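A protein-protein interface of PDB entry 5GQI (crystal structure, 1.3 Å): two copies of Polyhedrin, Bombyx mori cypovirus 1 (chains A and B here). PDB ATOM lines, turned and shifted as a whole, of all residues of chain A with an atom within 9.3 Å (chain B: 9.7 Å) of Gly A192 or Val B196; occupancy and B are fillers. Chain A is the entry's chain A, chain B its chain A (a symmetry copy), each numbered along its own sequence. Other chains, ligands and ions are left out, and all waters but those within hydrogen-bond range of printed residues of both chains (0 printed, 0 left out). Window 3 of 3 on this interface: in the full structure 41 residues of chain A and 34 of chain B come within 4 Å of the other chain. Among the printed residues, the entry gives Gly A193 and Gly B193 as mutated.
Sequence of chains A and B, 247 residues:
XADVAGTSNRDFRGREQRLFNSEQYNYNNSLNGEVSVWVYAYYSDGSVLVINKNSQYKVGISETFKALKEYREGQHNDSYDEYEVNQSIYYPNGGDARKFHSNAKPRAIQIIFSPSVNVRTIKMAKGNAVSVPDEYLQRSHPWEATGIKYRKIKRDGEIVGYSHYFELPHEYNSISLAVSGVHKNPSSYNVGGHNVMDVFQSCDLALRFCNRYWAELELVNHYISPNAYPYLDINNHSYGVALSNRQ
NZ of Lys A58 is in hydrogen-bond range of O of Phe B200, 3.3 Å away.
The side-chain amino group (NZ) of Lys A58 sits close to the side-chain sulfur (SG) of Cys A203, at 3.7 Å.
The side-chain amide oxygen (OD1) of Asn A190 is in hydrogen-bond range of the backbone NH (N) of Gly A192 (2.8 Å).
The side-chain amide nitrogen (ND2) of Asn A195 sits close to the backbone carbonyl oxygen (O) of Val A191, at 3.3 Å.
The side-chain sulfur (SG) of Cys A203 sits at hydrogen-bond distance from the backbone carbonyl oxygen (O) of Val A199 (3.6 Å).
Gln B201 touches Val A182 (CD to CG2, 3.4 Å).
CG2 of Val A191 touches CE of Met B197 (3.9 Å).
Gly A192 touches Val B196.
CE2 of Phe B200 touches CG1 of Val A199 (3.6 Å).
Phe A200 touches Phe B200.
SG of Cys A203 touches CD1 of Phe B200 (3.8 Å).
No residue of chain B comes within 4 Å of Asn A190.
Val A191 touches just one residue of chain B: Met B197.
Gly A192 touches just one residue of chain B: Val B196 (3.8 Å).
No residue of chain B comes within 4 Å of Gly A193.
Of the printed residues of chain B, Val A199 touches Phe B200.
Asn B195 touches none of the printed residues of chain A.
Val B196 touches just one residue of chain A: Gly A192.
Of the printed residues of chain A, Phe B200 touches Lys A58 (3.3 Å), Val A199 (3.6 Å), Phe A200 (3.5 Å) and Cys A203 (3.8 Å).
Printed residues of chain A within 4 Å of Gln B201: Val A182.
The nearest residue of chain A that does not touch Val B196 is Asn A190 (4.1 Å).
The nearest printed residue of chain A that does not touch Met B197 is Lys A58 (4.04 Å).
Of the 19 printed residues of chain A, 7 touch a printed residue of chain B.
Printed residues of chain A that touch a printed residue of chain B: Lys A58, Val A182, Val A191, Gly A192, Val A199, Phe A200 and Cys A203.
Hydrophobic or aromatic side chains of chain A within 4 Å of the printed part of chain B: Val A182, Val A191, Val A199 and Phe A200.
Of the 18 printed residues of chain B, 4 touch a printed residue of chain A.
Printed residues of chain B that touch a printed residue of chain A: Val B196, Met B197, Phe B200 and Gln B201.
Hydrophobic or aromatic side chains of chain B within 4 Å of the printed part of chain A: Val B196, Met B197 and Phe B200.
Among the printed residues, 7 pairs touch across the chains.
Among the printed residues, no Asp or Glu carboxylate lies within 4 Å of a Lys or Arg side-chain nitrogen of the other chain.
Lys A58 touches Phe B200, but with the chains exchanged Phe A200 does not touch Lys B58 (7.1 Å).
Gly A192 touches Val B196, but with the chains exchanged Val A196 does not touch Gly B192 (6.2 Å).
Phe A200 touches its own counterpart, Phe B200.
Cys A203 touches Phe B200, but with the chains exchanged Phe A200 does not touch Cys B203 (6.1 Å).
15 positions are printed for both chains.
Of the 7 pairs that touch across the chains among the printed residues, 1 has its exchanged pair printed and touching as well.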
ATOM      1  N   LEU A  31      13.150  32.348  35.684  1.00  0.00           N
ATOM      2  CA  LEU A  31      11.873  32.016  34.995  1.00  0.00           C
ATOM      3  C   LEU A  31      10.728  32.826  35.537  1.00  0.00           C
ATOM      4  O   LEU A  31       9.667  32.840  34.933  1.00  0.00           O
ATOM      5  CB  LEU A  31      11.619  30.503  35.126  1.00  0.00           C
ATOM      6  CG  LEU A  31      12.704  29.566  34.617  1.00  0.00           C
ATOM      7  CD1 LEU A  31      12.382  28.103  34.936  1.00  0.00           C
ATOM      8  CD2 LEU A  31      12.818  29.795  33.137  1.00  0.00           C
ATOM      9  N   TYR A  57       7.916  33.698  30.098  1.00  0.00           N
ATOM     10  CA  TYR A  57       8.094  32.421  29.401  1.00  0.00           C
ATOM     11  C   TYR A  57       8.392  32.527  27.892  1.00  0.00           C
ATOM     12  O   TYR A  57       9.342  31.860  27.410  1.00  0.00           O
ATOM     13  CB  TYR A  57       6.893  31.413  29.545  1.00  0.00           C
ATOM     14  CG  TYR A  57       6.455  31.258  30.999  1.00  0.00           C
ATOM     15  CD1 TYR A  57       7.335  30.751  31.948  1.00  0.00           C
ATOM     16  CD2 TYR A  57       5.198  31.719  31.405  1.00  0.00           C
ATOM     17  CE1 TYR A  57       6.914  30.652  33.288  1.00  0.00           C
ATOM     18  CE2 TYR A  57       4.749  31.567  32.720  1.00  0.00           C
ATOM     19  CZ  TYR A  57       5.653  31.051  33.653  1.00  0.00           C
ATOM     20  OH  TYR A  57       5.237  30.893  34.972  1.00  0.00           O
ATOM     21  N   LYS A  58       7.589  33.308  27.160  1.00  0.00           N
ATOM     22  CA  LYS A  58       7.740  33.450  25.729  1.00  0.00           C
ATOM     23  C   LYS A  58       6.987  34.709  25.364  1.00  0.00           C
ATOM     24  O   LYS A  58       6.043  35.114  26.100  1.00  0.00           O
ATOM     25  CB  LYS A  58       7.194  32.176  24.981  1.00  0.00           C
ATOM     26  CG  LYS A  58       5.661  31.945  25.171  1.00  0.00           C
ATOM     27  CD  LYS A  58       4.785  32.651  24.047  1.00  0.00           C
ATOM     28  CE  LYS A  58       3.305  32.430  24.289  1.00  0.00           C
ATOM     29  NZ  LYS A  58       2.506  33.052  23.123  1.00  0.00           N
ATOM     30  N   VAL A 182      11.630  32.808  23.079  1.00  0.00           N
ATOM     31  CA  VAL A 182      11.374  32.156  24.345  1.00  0.00           C
ATOM     32  C   VAL A 182      12.363  32.652  25.413  1.00  0.00           C
ATOM     33  O   VAL A 182      13.556  32.817  25.117  1.00  0.00           O
ATOM     34  CB  VAL A 182      11.515  30.591  24.125  1.00  0.00           C
ATOM     35  CG1 VAL A 182      11.350  29.820  25.427  1.00  0.00           C
ATOM     36  CG2 VAL A 182      10.415  30.093  23.172  1.00  0.00           C
ATOM     37  N   ASN A 185      15.969  29.408  29.534  1.00  0.00           N
ATOM     38  CA  ASN A 185      15.629  28.366  30.527  1.00  0.00           C
ATOM     39  C   ASN A 185      16.759  27.336  30.473  1.00  0.00           C
ATOM     40  O   ASN A 185      16.655  26.364  29.761  1.00  0.00           O
ATOM     41  CB  ASN A 185      14.290  27.658  30.290  1.00  0.00           C
ATOM     42  CG  ASN A 185      14.020  26.673  31.426  1.00  0.00           C
ATOM     43  OD1 ASN A 185      14.818  26.596  32.400  1.00  0.00           O
ATOM     44  ND2 ASN A 185      12.887  25.994  31.362  1.00  0.00           N
ATOM     45  N   SER A 188      16.400  21.976  33.417  1.00  0.00           N
ATOM     46  CA  SER A 188      15.650  20.895  32.769  1.00  0.00           C
ATOM     47  C   SER A 188      14.202  20.864  33.276  1.00  0.00           C
ATOM     48  O   SER A 188      13.477  19.882  33.055  1.00  0.00           O
ATOM     49  CB  SER A 188      16.349  19.518  32.944  1.00  0.00           C
ATOM     50  OG  SER A 188      16.735  19.337  34.330  1.00  0.00           O
ATOM     51  N   TYR A 189      13.730  21.944  33.918  1.00  0.00           N
ATOM     52  CA  TYR A 189      12.303  22.083  34.242  1.00  0.00           C
ATOM     53  C   TYR A 189      11.585  22.682  33.034  1.00  0.00           C
ATOM     54  O   TYR A 189      11.835  23.861  32.719  1.00  0.00           O
ATOM     55  CB  TYR A 189      12.104  22.961  35.485  1.00  0.00           C
ATOM     56  CG  TYR A 189      10.648  23.114  35.965  1.00  0.00           C
ATOM     57  CD1 TYR A 189      10.120  22.230  36.869  1.00  0.00           C
ATOM     58  CD2 TYR A 189       9.853  24.105  35.479  1.00  0.00           C
ATOM     59  CE1 TYR A 189       8.813  22.355  37.330  1.00  0.00           C
ATOM     60  CE2 TYR A 189       8.509  24.249  35.899  1.00  0.00           C
ATOM     61  CZ  TYR A 189       8.038  23.338  36.820  1.00  0.00           C
ATOM     62  OH  TYR A 189       6.722  23.494  37.234  1.00  0.00           O
ATOM     63  N   ASN A 190      10.742  21.947  32.351  1.00  0.00           N
ATOM     64  CA  ASN A 190      10.046  22.517  31.217  1.00  0.00           C
ATOM     65  C   ASN A 190       8.930  23.471  31.712  1.00  0.00           C
ATOM     66  O   ASN A 190       8.080  23.024  32.507  1.00  0.00           O
ATOM     67  CB  ASN A 190       9.369  21.372  30.477  1.00  0.00           C
ATOM     68  CG  ASN A 190       8.865  21.805  29.076  1.00  0.00           C
ATOM     69  OD1 ASN A 190       8.407  22.911  28.900  1.00  0.00           O
ATOM     70  ND2 ASN A 190       9.034  20.937  28.078  1.00  0.00           N
ATOM     71  N   VAL A 191       8.924  24.714  31.299  1.00  0.00           N
ATOM     72  CA  VAL A 191       7.834  25.616  31.769  1.00  0.00           C
ATOM     73  C   VAL A 191       6.504  25.256  31.199  1.00  0.00           C
ATOM     74  O   VAL A 191       5.498  25.701  31.766  1.00  0.00           O
ATOM     75  CB  VAL A 191       8.171  27.131  31.584  1.00  0.00           C
ATOM     76  CG1 VAL A 191       9.446  27.523  32.382  1.00  0.00           C
ATOM     77  CG2 VAL A 191       8.264  27.428  30.112  1.00  0.00           C
ATOM     78  N   GLY A 192       6.460  24.441  30.139  1.00  0.00           N
ATOM     79  CA  GLY A 192       5.218  23.890  29.577  1.00  0.00           C
ATOM     80  C   GLY A 192       4.881  22.507  30.037  1.00  0.00           C
ATOM     81  O   GLY A 192       4.006  21.849  29.461  1.00  0.00           O
ATOM     82  N   GLY A 193       5.487  22.030  31.155  1.00  0.00           N
ATOM     83  CA  GLY A 193       5.164  20.747  31.693  1.00  0.00           C
ATOM     84  C   GLY A 193       4.129  20.908  32.769  1.00  0.00           C
ATOM     85  O   GLY A 193       2.941  21.156  32.643  1.00  0.00           O
ATOM     86  N   HIS A 194       4.571  20.745  34.158  1.00  0.00           N
ATOM     87  CA  HIS A 194       3.712  21.036  35.263  1.00  0.00           C
ATOM     88  C   HIS A 194       3.141  22.445  35.259  1.00  0.00           C
ATOM     89  O   HIS A 194       2.085  22.742  35.841  1.00  0.00           O
ATOM     90  CB  HIS A 194       4.521  20.950  36.582  1.00  0.00           C
ATOM     91  CG  HIS A 194       4.540  19.588  37.185  1.00  0.00           C
ATOM     92  ND1 HIS A 194       5.181  19.349  38.387  1.00  0.00           N
ATOM     93  CD2 HIS A 194       3.980  18.416  36.773  1.00  0.00           C
ATOM     94  CE1 HIS A 194       4.972  18.058  38.723  1.00  0.00           C
ATOM     95  NE2 HIS A 194       4.269  17.475  37.746  1.00  0.00           N
ATOM     96  N   ASN A 195       3.903  23.312  34.579  1.00  0.00           N
ATOM     97  CA  ASN A 195       3.537  24.766  34.582  1.00  0.00           C
ATOM     98  C   ASN A 195       2.788  25.178  33.323  1.00  0.00           C
ATOM     99  O   ASN A 195       2.583  26.324  33.102  1.00  0.00           O
ATOM    100  CB  ASN A 195       4.840  25.547  34.808  1.00  0.00           C
ATOM    101  CG  ASN A 195       4.658  27.000  35.098  1.00  0.00           C
ATOM    102  OD1 ASN A 195       4.125  27.324  36.181  1.00  0.00           O
ATOM    103  ND2 ASN A 195       5.164  27.884  34.204  1.00  0.00           N
ATOM    104  N   VAL A 196       2.287  24.189  32.554  1.00  0.00           N
ATOM    105  CA  VAL A 196       1.631  24.514  31.262  1.00  0.00           C
ATOM    106  C   VAL A 196       0.527  25.532  31.380  1.00  0.00           C
ATOM    107  O   VAL A 196       0.444  26.435  30.528  1.00  0.00           O
ATOM    108  CB  VAL A 196       1.206  23.215  30.547  1.00  0.00           C
ATOM    109  CG1 VAL A 196       0.000  22.511  31.230  1.00  0.00           C
ATOM    110  CG2 VAL A 196       0.880  23.532  29.044  1.00  0.00           C
ATOM    111  N   MET A 197      -0.368  25.383  32.380  1.00  0.00           N
ATOM    112  CA  MET A 197      -1.480  26.352  32.439  1.00  0.00           C
ATOM    113  C   MET A 197      -1.017  27.737  32.807  1.00  0.00           C
ATOM    114  O   MET A 197      -1.666  28.720  32.390  1.00  0.00           O
ATOM    115  CB  MET A 197      -2.594  25.843  33.385  1.00  0.00           C
ATOM    116  CG  MET A 197      -3.286  24.570  32.830  1.00  0.00           C
ATOM    117  SD  MET A 197      -4.063  24.831  31.187  1.00  0.00           S
ATOM    118  CE  MET A 197      -5.405  25.881  31.668  1.00  0.00           C
ATOM    119  N   ASP A 198       0.122  27.865  33.495  1.00  0.00           N
ATOM    120  CA  ASP A 198       0.694  29.188  33.682  1.00  0.00           C
ATOM    121  C   ASP A 198       1.188  29.842  32.426  1.00  0.00           C
ATOM    122  O   ASP A 198       1.107  31.051  32.240  1.00  0.00           O
ATOM    123  CB  ASP A 198       1.899  29.064  34.714  1.00  0.00           C
ATOM    124  CG  ASP A 198       1.408  28.857  36.137  1.00  0.00           C
ATOM    125  OD1 ASP A 198       0.605  27.898  36.322  1.00  0.00           O
ATOM    126  OD2 ASP A 198       1.769  29.706  36.988  1.00  0.00           O
ATOM    127  N   VAL A 199       1.692  28.978  31.498  1.00  0.00           N
ATOM    128  CA  VAL A 199       2.101  29.528  30.194  1.00  0.00           C
ATOM    129  C   VAL A 199       0.855  29.943  29.421  1.00  0.00           C
ATOM    130  O   VAL A 199       0.835  31.017  28.793  1.00  0.00           O
ATOM    131  CB  VAL A 199       3.022  28.551  29.382  1.00  0.00           C
ATOM    132  CG1 VAL A 199       3.541  29.304  28.113  1.00  0.00           C
ATOM    133  CG2 VAL A 199       4.222  28.110  30.244  1.00  0.00           C
ATOM    134  N   PHE A 200      -0.231  29.145  29.496  1.00  0.00           N
ATOM    135  CA  PHE A 200      -1.464  29.622  28.894  1.00  0.00           C
ATOM    136  C   PHE A 200      -1.930  30.955  29.481  1.00  0.00           C
ATOM    137  O   PHE A 200      -2.375  31.864  28.744  1.00  0.00           O
ATOM    138  CB  PHE A 200      -2.563  28.558  28.987  1.00  0.00           C
ATOM    139  CG  PHE A 200      -2.504  27.502  27.928  1.00  0.00           C
ATOM    140  CD1 PHE A 200      -2.723  27.842  26.588  1.00  0.00           C
ATOM    141  CD2 PHE A 200      -2.155  26.190  28.278  1.00  0.00           C
ATOM    142  CE1 PHE A 200      -2.667  26.855  25.612  1.00  0.00           C
ATOM    143  CE2 PHE A 200      -2.088  25.154  27.280  1.00  0.00           C
ATOM    144  CZ  PHE A 200      -2.313  25.551  25.940  1.00  0.00           C
ATOM    145  N   CYS A 203      -0.209  33.962  28.031  1.00  0.00           N
ATOM    146  CA  CYS A 203      -0.672  34.455  26.720  1.00  0.00           C
ATOM    147  C   CYS A 203      -1.728  35.558  26.983  1.00  0.00           C
ATOM    148  O   CYS A 203      -1.808  36.499  26.187  1.00  0.00           O
ATOM    149  CB  CYS A 203      -1.321  33.303  25.979  1.00  0.00           C
ATOM    150  SG  CYS A 203      -0.083  32.051  25.503  1.00  0.00           S
ATOM    151  N   GLN B  56       1.269  27.172  11.993  1.00  0.00           N
ATOM    152  CA  GLN B  56       1.613  25.745  12.193  1.00  0.00           C
ATOM    153  C   GLN B  56       0.781  25.147  13.342  1.00  0.00           C
ATOM    154  O   GLN B  56       0.354  25.884  14.251  1.00  0.00           O
ATOM    155  CB  GLN B  56       3.074  25.768  12.616  1.00  0.00           C
ATOM    156  CG  GLN B  56       3.797  24.443  12.399  1.00  0.00           C
ATOM    157  CD  GLN B  56       5.293  24.551  12.653  1.00  0.00           C
ATOM    158  OE1 GLN B  56       5.826  25.607  13.082  1.00  0.00           O
ATOM    159  NE2 GLN B  56       6.033  23.463  12.345  1.00  0.00           N
ATOM    160  N   TYR B  57       0.594  23.835  13.288  1.00  0.00           N
ATOM    161  CA  TYR B  57       0.011  23.031  14.366  1.00  0.00           C
ATOM    162  C   TYR B  57      -1.511  23.185  14.558  1.00  0.00           C
ATOM    163  O   TYR B  57      -2.219  22.153  14.663  1.00  0.00           O
ATOM    164  CB  TYR B  57       0.660  23.251  15.784  1.00  0.00           C
ATOM    165  CG  TYR B  57       2.184  23.180  15.726  1.00  0.00           C
ATOM    166  CD1 TYR B  57       2.819  22.009  15.328  1.00  0.00           C
ATOM    167  CD2 TYR B  57       2.948  24.325  15.978  1.00  0.00           C
ATOM    168  CE1 TYR B  57       4.225  21.985  15.252  1.00  0.00           C
ATOM    169  CE2 TYR B  57       4.346  24.293  15.965  1.00  0.00           C
ATOM    170  CZ  TYR B  57       4.959  23.102  15.564  1.00  0.00           C
ATOM    171  OH  TYR B  57       6.349  23.040  15.536  1.00  0.00           O
ATOM    172  N   LYS B  58      -1.997  24.429  14.639  1.00  0.00           N
ATOM    173  CA  LYS B  58      -3.399  24.701  14.864  1.00  0.00           C
ATOM    174  C   LYS B  58      -3.609  26.137  14.443  1.00  0.00           C
ATOM    175  O   LYS B  58      -2.638  26.946  14.460  1.00  0.00           O
ATOM    176  CB  LYS B  58      -3.781  24.446  16.371  1.00  0.00           C
ATOM    177  CG  LYS B  58      -3.054  25.398  17.373  1.00  0.00           C
ATOM    178  CD  LYS B  58      -3.873  26.728  17.668  1.00  0.00           C
ATOM    179  CE  LYS B  58      -3.116  27.637  18.617  1.00  0.00           C
ATOM    180  NZ  LYS B  58      -3.993  28.865  18.944  1.00  0.00           N
ATOM    181  N   TYR B 189       3.352  11.240  17.796  1.00  0.00           N
ATOM    182  CA  TYR B 189       4.131  12.323  18.415  1.00  0.00           C
ATOM    183  C   TYR B 189       3.188  13.485  18.726  1.00  0.00           C
ATOM    184  O   TYR B 189       2.689  14.116  17.775  1.00  0.00           O
ATOM    185  CB  TYR B 189       5.271  12.777  17.493  1.00  0.00           C
ATOM    186  CG  TYR B 189       6.204  13.858  18.072  1.00  0.00           C
ATOM    187  CD1 TYR B 189       7.319  13.501  18.785  1.00  0.00           C
ATOM    188  CD2 TYR B 189       5.923  15.179  17.916  1.00  0.00           C
ATOM    189  CE1 TYR B 189       8.185  14.458  19.305  1.00  0.00           C
ATOM    190  CE2 TYR B 189       6.762  16.184  18.455  1.00  0.00           C
ATOM    191  CZ  TYR B 189       7.876  15.764  19.151  1.00  0.00           C
ATOM    192  OH  TYR B 189       8.699  16.756  19.665  1.00  0.00           O
ATOM    193  N   ASN B 190       2.915  13.781  19.972  1.00  0.00           N
ATOM    194  CA  ASN B 190       2.038  14.893  20.271  1.00  0.00           C
ATOM    195  C   ASN B 190       2.787  16.230  20.039  1.00  0.00           C
ATOM    196  O   ASN B 190       3.867  16.414  20.635  1.00  0.00           O
ATOM    197  CB  ASN B 190       1.696  14.817  21.753  1.00  0.00           C
ATOM    198  CG  ASN B 190       0.516  15.754  22.124  1.00  0.00           C
ATOM    199  OD1 ASN B 190       0.398  16.836  21.594  1.00  0.00           O
ATOM    200  ND2 ASN B 190      -0.386  15.278  22.983  1.00  0.00           N
ATOM    201  N   VAL B 191       2.278  17.111  19.215  1.00  0.00           N
ATOM    202  CA  VAL B 191       3.000  18.400  19.015  1.00  0.00           C
ATOM    203  C   VAL B 191       2.961  19.275  20.222  1.00  0.00           C
ATOM    204  O   VAL B 191       3.791  20.190  20.293  1.00  0.00           O
ATOM    205  CB  VAL B 191       2.558  19.155  17.719  1.00  0.00           C
ATOM    206  CG1 VAL B 191       2.826  18.294  16.451  1.00  0.00           C
ATOM    207  CG2 VAL B 191       1.122  19.575  17.871  1.00  0.00           C
ATOM    208  N   GLY B 192       2.069  19.003  21.181  1.00  0.00           N
ATOM    209  CA  GLY B 192       2.027  19.690  22.482  1.00  0.00           C
ATOM    210  C   GLY B 192       2.712  18.963  23.595  1.00  0.00           C
ATOM    211  O   GLY B 192       2.542  19.312  24.770  1.00  0.00           O
ATOM    212  N   GLY B 193       3.595  17.981  23.283  1.00  0.00           N
ATOM    213  CA  GLY B 193       4.338  17.292  24.289  1.00  0.00           C
ATOM    214  C   GLY B 193       5.683  17.944  24.445  1.00  0.00           C
ATOM    215  O   GLY B 193       5.948  19.011  24.975  1.00  0.00           O
ATOM    216  N   HIS B 194       6.844  17.228  23.906  1.00  0.00           N
ATOM    217  CA  HIS B 194       8.142  17.826  23.853  1.00  0.00           C
ATOM    218  C   HIS B 194       8.192  19.149  23.107  1.00  0.00           C
ATOM    219  O   HIS B 194       9.067  20.005  23.316  1.00  0.00           O
ATOM    220  CB  HIS B 194       9.104  16.901  23.065  1.00  0.00           C
ATOM    221  CG  HIS B 194       9.798  15.896  23.917  1.00  0.00           C
ATOM    222  ND1 HIS B 194      10.724  15.021  23.377  1.00  0.00           N
ATOM    223  CD2 HIS B 194       9.724  15.648  25.254  1.00  0.00           C
ATOM    224  CE1 HIS B 194      11.240  14.285  24.384  1.00  0.00           C
ATOM    225  NE2 HIS B 194      10.629  14.634  25.521  1.00  0.00           N
ATOM    226  N   ASN B 195       7.207  19.276  22.206  1.00  0.00           N
ATOM    227  CA  ASN B 195       7.189  20.474  21.306  1.00  0.00           C
ATOM    228  C   ASN B 195       6.229  21.550  21.792  1.00  0.00           C
ATOM    229  O   ASN B 195       5.977  22.479  21.100  1.00  0.00           O
ATOM    230  CB  ASN B 195       6.873  19.959  19.894  1.00  0.00           C
ATOM    231  CG  ASN B 195       7.059  20.962  18.804  1.00  0.00           C
ATOM    232  OD1 ASN B 195       8.221  21.343  18.545  1.00  0.00           O
ATOM    233  ND2 ASN B 195       5.961  21.332  18.102  1.00  0.00           N
ATOM    234  N   VAL B 196       5.783  21.449  23.062  1.00  0.00           N
ATOM    235  CA  VAL B 196       4.770  22.407  23.571  1.00  0.00           C
ATOM    236  C   VAL B 196       5.156  23.852  23.394  1.00  0.00           C
ATOM    237  O   VAL B 196       4.298  24.664  23.003  1.00  0.00           O
ATOM    238  CB  VAL B 196       4.379  22.040  25.017  1.00  0.00           C
ATOM    239  CG1 VAL B 196       5.502  22.347  26.048  1.00  0.00           C
ATOM    240  CG2 VAL B 196       3.056  22.791  25.405  1.00  0.00           C
ATOM    241  N   MET B 197       6.412  24.217  23.728  1.00  0.00           N
ATOM    242  CA  MET B 197       6.751  25.649  23.610  1.00  0.00           C
ATOM    243  C   MET B 197       6.796  26.114  22.177  1.00  0.00           C
ATOM    244  O   MET B 197       6.531  27.308  21.923  1.00  0.00           O
ATOM    245  CB  MET B 197       8.069  25.959  24.360  1.00  0.00           C
ATOM    246  CG  MET B 197       7.917  25.774  25.894  1.00  0.00           C
ATOM    247  SD  MET B 197       6.624  26.853  26.624  1.00  0.00           S
ATOM    248  CE  MET B 197       7.427  28.421  26.453  1.00  0.00           C
ATOM    249  N   ASP B 198       7.033  25.209  21.223  1.00  0.00           N
ATOM    250  CA  ASP B 198       6.878  25.590  19.829  1.00  0.00           C
ATOM    251  C   ASP B 198       5.469  25.897  19.416  1.00  0.00           C
ATOM    252  O   ASP B 198       5.201  26.766  18.594  1.00  0.00           O
ATOM    253  CB  ASP B 198       7.440  24.406  18.927  1.00  0.00           C
ATOM    254  CG  ASP B 198       8.959  24.347  18.949  1.00  0.00           C
ATOM    255  OD1 ASP B 198       9.504  24.294  20.089  1.00  0.00           O
ATOM    256  OD2 ASP B 198       9.544  24.447  17.843  1.00  0.00           O
ATOM    257  N   VAL B 199       4.517  25.161  20.058  1.00  0.00           N
ATOM    258  CA  VAL B 199       3.103  25.475  19.787  1.00  0.00           C
ATOM    259  C   VAL B 199       2.768  26.823  20.414  1.00  0.00           C
ATOM    260  O   VAL B 199       2.080  27.650  19.790  1.00  0.00           O
ATOM    261  CB  VAL B 199       2.128  24.333  20.242  1.00  0.00           C
ATOM    262  CG1 VAL B 199       0.688  24.687  19.742  1.00  0.00           C
ATOM    263  CG2 VAL B 199       2.565  22.984  19.635  1.00  0.00           C
ATOM    264  N   PHE B 200       3.292  27.104  21.625  1.00  0.00           N
ATOM    265  CA  PHE B 200       3.106  28.448  22.147  1.00  0.00           C
ATOM    266  C   PHE B 200       3.678  29.524  21.224  1.00  0.00           C
ATOM    267  O   PHE B 200       3.052  30.584  21.003  1.00  0.00           O
ATOM    268  CB  PHE B 200       3.678  28.566  23.564  1.00  0.00           C
ATOM    269  CG  PHE B 200       2.775  28.064  24.648  1.00  0.00           C
ATOM    270  CD1 PHE B 200       1.564  28.717  24.909  1.00  0.00           C
ATOM    271  CD2 PHE B 200       3.115  26.897  25.346  1.00  0.00           C
ATOM    272  CE1 PHE B 200       0.734  28.246  25.917  1.00  0.00           C
ATOM    273  CE2 PHE B 200       2.264  26.390  26.392  1.00  0.00           C
ATOM    274  CZ  PHE B 200       1.050  27.084  26.612  1.00  0.00           C
ATOM    275  N   GLN B 201       4.905  29.302  20.723  1.00  0.00           N
ATOM    276  CA  GLN B 201       5.414  30.288  19.716  1.00  0.00           C
ATOM    277  C   GLN B 201       4.567  30.382  18.456  1.00  0.00           C
ATOM    278  O   GLN B 201       4.455  31.471  17.956  1.00  0.00           O
ATOM    279  CB  GLN B 201       6.840  29.894  19.313  1.00  0.00           C
ATOM    280  CG  GLN B 201       7.850  30.052  20.491  1.00  0.00           C
ATOM    281  CD  GLN B 201       9.289  29.969  19.963  1.00  0.00           C
ATOM    282  OE1 GLN B 201       9.877  28.873  19.862  1.00  0.00           O
ATOM    283  NE2 GLN B 201       9.854  31.183  19.604  1.00  0.00           N
ATOM    284  N   SER B 202       3.940  29.271  18.071  1.00  0.00           N
ATOM    285  CA  SER B 202       3.075  29.339  16.887  1.00  0.00           C
ATOM    286  C   SER B 202       1.905  30.290  17.114  1.00  0.00           C
ATOM    287  O   SER B 202       1.394  30.877  16.145  1.00  0.00           O
ATOM    288  CB  SER B 202       2.595  27.956  16.375  1.00  0.00           C
ATOM    289  OG  SER B 202       1.478  27.450  17.208  1.00  0.00           O
ATOM    290  N   CYS B 203       1.430  30.459  18.366  1.00  0.00           N
ATOM    291  CA  CYS B 203       0.315  31.386  18.641  1.00  0.00           C
ATOM    292  C   CYS B 203       0.811  32.820  18.329  1.00  0.00           C
ATOM    293  O   CYS B 203       0.001  33.641  17.891  1.00  0.00           O
ATOM    294  CB  CYS B 203      -0.037  31.284  20.113  1.00  0.00           C
ATOM    295  SG  CYS B 203      -0.781  29.663  20.496  1.00  0.00           S
